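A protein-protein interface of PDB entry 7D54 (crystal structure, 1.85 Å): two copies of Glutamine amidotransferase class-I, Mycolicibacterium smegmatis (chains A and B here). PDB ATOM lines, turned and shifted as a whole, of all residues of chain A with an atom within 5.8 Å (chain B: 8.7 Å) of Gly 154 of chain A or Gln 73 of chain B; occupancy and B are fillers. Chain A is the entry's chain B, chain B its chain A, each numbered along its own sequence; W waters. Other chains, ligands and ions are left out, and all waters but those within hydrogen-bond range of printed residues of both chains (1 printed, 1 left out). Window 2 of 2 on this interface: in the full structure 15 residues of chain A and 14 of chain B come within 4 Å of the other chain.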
ATOM      1  N   THR A 150      12.285   0.540  21.365  1.00  0.00           N
ATOM      2  CA  THR A 150      11.630   1.654  22.033  1.00  0.00           C
ATOM      3  C   THR A 150      12.545   2.854  21.868  1.00  0.00           C
ATOM      4  O   THR A 150      13.763   2.728  22.011  1.00  0.00           O
ATOM      5  CB  THR A 150      11.370   1.375  23.518  1.00  0.00           C
ATOM      6  OG1 THR A 150      12.587   1.483  24.251  1.00  0.00           O
ATOM      7  CG2 THR A 150      10.809   0.026  23.678  1.00  0.00           C
ATOM      8  N   VAL A 151      11.967   3.989  21.498  1.00  0.00           N
ATOM      9  CA  VAL A 151      12.774   5.183  21.208  1.00  0.00           C
ATOM     10  C   VAL A 151      13.515   5.613  22.463  1.00  0.00           C
ATOM     11  O   VAL A 151      12.889   5.705  23.539  1.00  0.00           O
ATOM     12  CB  VAL A 151      11.875   6.312  20.699  1.00  0.00           C
ATOM     13  CG1 VAL A 151      12.669   7.583  20.505  1.00  0.00           C
ATOM     14  CG2 VAL A 151      11.191   5.850  19.389  1.00  0.00           C
ATOM     15  N   PRO A 152      14.819   5.874  22.399  1.00  0.00           N
ATOM     16  CA  PRO A 152      15.568   6.189  23.631  1.00  0.00           C
ATOM     17  C   PRO A 152      15.137   7.520  24.223  1.00  0.00           C
ATOM     18  O   PRO A 152      14.639   8.409  23.505  1.00  0.00           O
ATOM     19  CB  PRO A 152      17.031   6.231  23.176  1.00  0.00           C
ATOM     20  CG  PRO A 152      16.982   6.510  21.732  1.00  0.00           C
ATOM     21  CD  PRO A 152      15.674   5.942  21.195  1.00  0.00           C
ATOM     22  N   PRO A 153      15.313   7.687  25.540  1.00  0.00           N
ATOM     23  CA  PRO A 153      14.973   8.967  26.171  1.00  0.00           C
ATOM     24  C   PRO A 153      15.707  10.111  25.486  1.00  0.00           C
ATOM     25  O   PRO A 153      16.866   9.980  25.062  1.00  0.00           O
ATOM     26  CB  PRO A 153      15.419   8.783  27.624  1.00  0.00           C
ATOM     27  CG  PRO A 153      16.650   7.936  27.471  1.00  0.00           C
ATOM     28  CD  PRO A 153      16.266   6.916  26.360  1.00  0.00           C
ATOM     29  N   GLY A 154      15.009  11.242  25.363  1.00  0.00           N
ATOM     30  CA  GLY A 154      15.545  12.420  24.698  1.00  0.00           C
ATOM     31  C   GLY A 154      15.455  12.419  23.185  1.00  0.00           C
ATOM     32  O   GLY A 154      15.679  13.471  22.551  1.00  0.00           O
ATOM     33  N   ALA A 155      15.147  11.292  22.578  1.00  0.00           N
ATOM     34  CA  ALA A 155      15.020  11.222  21.131  1.00  0.00           C
ATOM     35  C   ALA A 155      13.600  11.563  20.712  1.00  0.00           C
ATOM     36  O   ALA A 155      12.666  11.507  21.505  1.00  0.00           O
ATOM     37  CB  ALA A 155      15.402   9.833  20.628  1.00  0.00           C
ATOM     38  N   THR A 156      13.447  11.941  19.448  1.00  0.00           N
ATOM     39  CA  THR A 156      12.148  12.240  18.869  1.00  0.00           C
ATOM     40  C   THR A 156      11.857  11.250  17.764  1.00  0.00           C
ATOM     41  O   THR A 156      12.600  11.202  16.783  1.00  0.00           O
ATOM     42  CB  THR A 156      12.124  13.650  18.285  1.00  0.00           C
ATOM     43  OG1 THR A 156      12.535  14.555  19.302  1.00  0.00           O
ATOM     44  CG2 THR A 156      10.736  14.007  17.797  1.00  0.00           C
ATOM     45  N   VAL A 169      15.294  10.744  15.740  1.00  0.00           N
ATOM     46  CA  VAL A 169      16.445  11.617  15.764  1.00  0.00           C
ATOM     47  C   VAL A 169      16.846  11.840  17.208  1.00  0.00           C
ATOM     48  O   VAL A 169      15.994  12.027  18.092  1.00  0.00           O
ATOM     49  CB  VAL A 169      16.138  12.944  15.050  1.00  0.00           C
ATOM     50  CG1 VAL A 169      17.339  13.883  15.193  1.00  0.00           C
ATOM     51  CG2 VAL A 169      15.815  12.676  13.596  1.00  0.00           C
ATOM     52  N   LEU A 170      18.151  11.858  17.441  1.00  0.00           N
ATOM     53  CA  LEU A 170      18.720  12.177  18.744  1.00  0.00           C
ATOM     54  C   LEU A 170      19.970  12.974  18.412  1.00  0.00           C
ATOM     55  O   LEU A 170      20.959  12.413  17.954  1.00  0.00           O
ATOM     56  CB  LEU A 170      19.035  10.928  19.551  1.00  0.00           C
ATOM     57  CG  LEU A 170      19.713  11.211  20.893  1.00  0.00           C
ATOM     58  CD1 LEU A 170      18.729  11.961  21.786  1.00  0.00           C
ATOM     59  CD2 LEU A 170      20.179   9.902  21.552  1.00  0.00           C
ATOM     60  N   ALA B  47       7.469   9.200  35.360  1.00  0.00           N
ATOM     61  CA  ALA B  47       8.849   9.197  34.873  1.00  0.00           C
ATOM     62  C   ALA B  47       9.823   9.777  35.907  1.00  0.00           C
ATOM     63  O   ALA B  47       9.515  10.733  36.625  1.00  0.00           O
ATOM     64  CB  ALA B  47       8.948   9.971  33.545  1.00  0.00           C
ATOM     65  N   PRO B  69       2.331   1.963  30.391  1.00  0.00           N
ATOM     66  CA  PRO B  69       2.949   1.014  29.452  1.00  0.00           C
ATOM     67  C   PRO B  69       4.407   0.807  29.814  1.00  0.00           C
ATOM     68  O   PRO B  69       5.177   1.766  29.945  1.00  0.00           O
ATOM     69  CB  PRO B  69       2.798   1.680  28.075  1.00  0.00           C
ATOM     70  CG  PRO B  69       2.014   2.987  28.316  1.00  0.00           C
ATOM     71  CD  PRO B  69       2.110   3.288  29.785  1.00  0.00           C
ATOM     72  N   VAL B  70       4.791  -0.467  29.932  1.00  0.00           N
ATOM     73  CA  VAL B  70       6.167  -0.821  30.246  1.00  0.00           C
ATOM     74  C   VAL B  70       7.138  -0.378  29.164  1.00  0.00           C
ATOM     75  O   VAL B  70       8.346  -0.294  29.421  1.00  0.00           O
ATOM     76  CB  VAL B  70       6.241  -2.354  30.508  1.00  0.00           C
ATOM     77  CG1 VAL B  70       6.211  -3.111  29.222  1.00  0.00           C
ATOM     78  CG2 VAL B  70       7.483  -2.660  31.293  1.00  0.00           C
ATOM     79  N   TYR B  71       6.637  -0.032  27.976  1.00  0.00           N
ATOM     80  CA  TYR B  71       7.466   0.377  26.852  1.00  0.00           C
ATOM     81  C   TYR B  71       7.468   1.889  26.657  1.00  0.00           C
ATOM     82  O   TYR B  71       8.040   2.382  25.676  1.00  0.00           O
ATOM     83  CB  TYR B  71       6.994  -0.291  25.555  1.00  0.00           C
ATOM     84  CG  TYR B  71       5.507  -0.194  25.355  1.00  0.00           C
ATOM     85  CD1 TYR B  71       4.922   0.967  24.862  1.00  0.00           C
ATOM     86  CD2 TYR B  71       4.680  -1.236  25.723  1.00  0.00           C
ATOM     87  CE1 TYR B  71       3.538   1.059  24.708  1.00  0.00           C
ATOM     88  CE2 TYR B  71       3.322  -1.152  25.571  1.00  0.00           C
ATOM     89  CZ  TYR B  71       2.752  -0.004  25.070  1.00  0.00           C
ATOM     90  OH  TYR B  71       1.375   0.062  24.922  1.00  0.00           O
ATOM     91  N   GLU B  72       6.875   2.626  27.584  1.00  0.00           N
ATOM     92  CA  GLU B  72       6.827   4.080  27.486  1.00  0.00           C
ATOM     93  C   GLU B  72       8.238   4.657  27.420  1.00  0.00           C
ATOM     94  O   GLU B  72       9.088   4.368  28.261  1.00  0.00           O
ATOM     95  CB  GLU B  72       6.057   4.636  28.682  1.00  0.00           C
ATOM     96  CG  GLU B  72       5.849   6.145  28.683  1.00  0.00           C
ATOM     97  CD  GLU B  72       4.947   6.585  27.572  1.00  0.00           C
ATOM     98  OE1 GLU B  72       4.240   5.706  27.008  1.00  0.00           O
ATOM     99  OE2 GLU B  72       4.939   7.809  27.275  1.00  0.00           O
ATOM    100  N   GLN B  73       8.478   5.510  26.430  1.00  0.00           N
ATOM    101  CA  GLN B  73       9.825   6.023  26.205  1.00  0.00           C
ATOM    102  C   GLN B  73      10.443   6.584  27.471  1.00  0.00           C
ATOM    103  O   GLN B  73      11.631   6.380  27.732  1.00  0.00           O
ATOM    104  CB  GLN B  73       9.783   7.089  25.097  1.00  0.00           C
ATOM    105  CG  GLN B  73      11.036   7.949  24.995  1.00  0.00           C
ATOM    106  CD  GLN B  73      10.892   9.077  23.981  1.00  0.00           C
ATOM    107  OE1 GLN B  73       9.785   9.439  23.573  1.00  0.00           O
ATOM    108  NE2 GLN B  73      12.004   9.616  23.564  1.00  0.00           N
ATOM    109  N   SER B  74       9.686   7.393  28.226  1.00  0.00           N
ATOM    110  CA  SER B  74      10.286   8.052  29.376  1.00  0.00           C
ATOM    111  C   SER B  74      10.342   7.158  30.606  1.00  0.00           C
ATOM    112  O   SER B  74      11.051   7.509  31.564  1.00  0.00           O
ATOM    113  CB  SER B  74       9.550   9.331  29.737  1.00  0.00           C
ATOM    114  OG  SER B  74       8.218   9.066  30.116  1.00  0.00           O
ATOM    115  N   LEU B  75       9.639   6.020  30.586  1.00  0.00           N
ATOM    116  CA  LEU B  75       9.787   5.037  31.651  1.00  0.00           C
ATOM    117  C   LEU B  75      10.981   4.150  31.349  1.00  0.00           C
ATOM    118  O   LEU B  75      11.875   4.015  32.185  1.00  0.00           O
ATOM    119  CB  LEU B  75       8.508   4.213  31.828  1.00  0.00           C
ATOM    120  CG  LEU B  75       7.250   5.041  32.122  1.00  0.00           C
ATOM    121  CD1 LEU B  75       6.042   4.154  32.390  1.00  0.00           C
ATOM    122  CD2 LEU B  75       7.462   6.064  33.261  1.00  0.00           C
ATOM    123  N   VAL B  76      11.041   3.576  30.133  1.00  0.00           N
ATOM    124  CA  VAL B  76      12.241   2.834  29.725  1.00  0.00           C
ATOM    125  C   VAL B  76      13.468   3.729  29.882  1.00  0.00           C
ATOM    126  O   VAL B  76      14.576   3.284  30.216  1.00  0.00           O
ATOM    127  CB  VAL B  76      12.106   2.330  28.271  1.00  0.00           C
ATOM    128  CG1 VAL B  76      13.423   1.648  27.868  1.00  0.00           C
ATOM    129  CG2 VAL B  76      10.939   1.357  28.093  1.00  0.00           C
ATOM    130  N   GLY B  77      13.294   5.008  29.586  1.00  0.00           N
ATOM    131  CA  GLY B  77      14.359   5.956  29.715  1.00  0.00           C
ATOM    132  C   GLY B  77      14.752   6.255  31.129  1.00  0.00           C
ATOM    133  O   GLY B  77      15.840   6.791  31.316  1.00  0.00           O
ATOM    134  N   THR B  78      13.952   5.841  32.120  1.00  0.00           N
ATOM    135  CA  THR B  78      14.308   6.005  33.526  1.00  0.00           C
ATOM    136  C   THR B  78      14.156   4.689  34.274  1.00  0.00           C
ATOM    137  O   THR B  78      14.954   3.772  34.048  1.00  0.00           O
ATOM    138  CB  THR B  78      13.497   7.135  34.185  1.00  0.00           C
ATOM    139  OG1 THR B  78      12.100   6.845  34.202  1.00  0.00           O
ATOM    140  CG2 THR B  78      13.738   8.454  33.412  1.00  0.00           C
ATOM    141  N   TRP B  79      13.144   4.561  35.143  1.00  0.00           N
ATOM    142  CA  TRP B  79      13.196   3.479  36.135  1.00  0.00           C
ATOM    143  C   TRP B  79      12.842   2.101  35.593  1.00  0.00           C
ATOM    144  O   TRP B  79      13.170   1.089  36.244  1.00  0.00           O
ATOM    145  CB  TRP B  79      12.286   3.790  37.318  1.00  0.00           C
ATOM    146  CG  TRP B  79      10.821   4.027  37.033  1.00  0.00           C
ATOM    147  CD1 TRP B  79      10.193   5.256  36.856  1.00  0.00           C
ATOM    148  CD2 TRP B  79       9.784   3.040  36.942  1.00  0.00           C
ATOM    149  NE1 TRP B  79       8.846   5.076  36.675  1.00  0.00           N
ATOM    150  CE2 TRP B  79       8.566   3.727  36.710  1.00  0.00           C
ATOM    151  CE3 TRP B  79       9.763   1.640  37.030  1.00  0.00           C
ATOM    152  CZ2 TRP B  79       7.345   3.055  36.537  1.00  0.00           C
ATOM    153  CZ3 TRP B  79       8.520   0.979  36.896  1.00  0.00           C
ATOM    154  CH2 TRP B  79       7.345   1.687  36.671  1.00  0.00           C
ATOM    155  N   VAL B  80      12.176   2.012  34.443  1.00  0.00           N
ATOM    156  CA  VAL B  80      11.887   0.680  33.903  1.00  0.00           C
ATOM    157  C   VAL B  80      13.169  -0.051  33.533  1.00  0.00           C
ATOM    158  O   VAL B  80      13.324  -1.256  33.807  1.00  0.00           O
ATOM    159  CB  VAL B  80      10.931   0.756  32.703  1.00  0.00           C
ATOM    160  CG1 VAL B  80      11.006  -0.531  31.878  1.00  0.00           C
ATOM    161  CG2 VAL B  80       9.501   0.969  33.209  1.00  0.00           C
ATOM    162  N   THR B  81      14.103   0.648  32.906  1.00  0.00           N
ATOM    163  CA  THR B  81      15.382   0.028  32.585  1.00  0.00           C
ATOM    164  C   THR B  81      16.162  -0.329  33.849  1.00  0.00           C
ATOM    165  O   THR B  81      16.806  -1.394  33.905  1.00  0.00           O
ATOM    166  CB  THR B  81      16.191   0.949  31.672  1.00  0.00           C
ATOM    167  OG1 THR B  81      15.570   1.003  30.382  1.00  0.00           O
ATOM    168  CG2 THR B  81      17.600   0.432  31.516  1.00  0.00           C
ATOM    169  N   GLN B 109      10.163  -7.902  28.478  1.00  0.00           N
ATOM    170  CA  GLN B 109      11.039  -6.887  27.882  1.00  0.00           C
ATOM    171  C   GLN B 109      12.490  -7.053  28.342  1.00  0.00           C
ATOM    172  O   GLN B 109      13.433  -6.891  27.553  1.00  0.00           O
ATOM    173  CB  GLN B 109      10.489  -5.512  28.264  1.00  0.00           C
ATOM    174  CG  GLN B 109      10.942  -4.306  27.424  1.00  0.00           C
ATOM    175  CD  GLN B 109      10.034  -3.082  27.677  1.00  0.00           C
ATOM    176  OE1 GLN B 109       9.119  -2.797  26.906  1.00  0.00           O
ATOM    177  NE2 GLN B 109      10.296  -2.364  28.756  1.00  0.00           N
HETATM  178  O   HOH W   1      13.378   4.875  25.912  1.00  0.00           O
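O of Pro 152 of chain A lies within hydrogen-bond range of NE2 of Gln 73 of chain B (2.9 Å). O of Ala 155 of chain A is in hydrogen-bond range of NE2 of Gln 73 of chain B, 2.9 Å away.
Thr 150 of chain A touches Val 76 of chain B. Val 151 of chain A touches Gln 73 of chain B (O to CG, 3.3 Å). CB of Pro 153 of chain A touches CA of Gly 77 of chain B (3.7 Å). N of Gly 154 of chain A touches NE2 of Gln 73 of chain B (3.9 Å).
No position is printed for both chains. Of the 6 pairs that touch across the chains among the printed residues, none has its exchanged pair printed and touching as well.
Water W1 lies within hydrogen-bond range of O of Val 151 of chain A (2.6 Å) and O of Gln 73 of chain B (2.9 Å).
Printed residues of chain B within 4 Å of Thr 150 of chain A: Val 76. Printed residues of chain B within 4 Å of Val 151 of chain A: Gln 73 (3.3 Å). Of chain B, only Gln 73 (2.9 Å) comes within 4 Å of Ala 155 of chain A. Ala 47 of chain B touches none of the printed residues of chain A. Tyr 71 of chain B touches none of the printed residues of chain A. Of the printed residues of chain A, Gln 73 of chain B touches Val 151, Pro 152, Gly 154 and Ala 155. Printed residues of chain A within 4 Å of Val 76 of chain B: Thr 150. The nearest residue of chain B that does not touch Gly 154 of chain A is Gly 77 of chain B (6.9 Å). The nearest printed residue of chain B that does not touch Thr 150 of chain A is Tyr 71 of chain B (4.1 Å).
Of the 9 printed residues of chain A, 6 touch a printed residue of chain B. Printed residues of chain A that touch a printed residue of chain B: Thr 150, Val 151, Pro 152, Pro 153, Gly 154 and Ala 155. Among the printed residues, no Asp or Glu carboxylate lies within 4 Å of a Lys or Arg side-chain nitrogen of the other chain.
The backbone carbonyl oxygen of Val 76 of chain B is in hydrogen-bond range of the side-chain hydroxyl of Thr 81 of chain B (2.5 Å).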
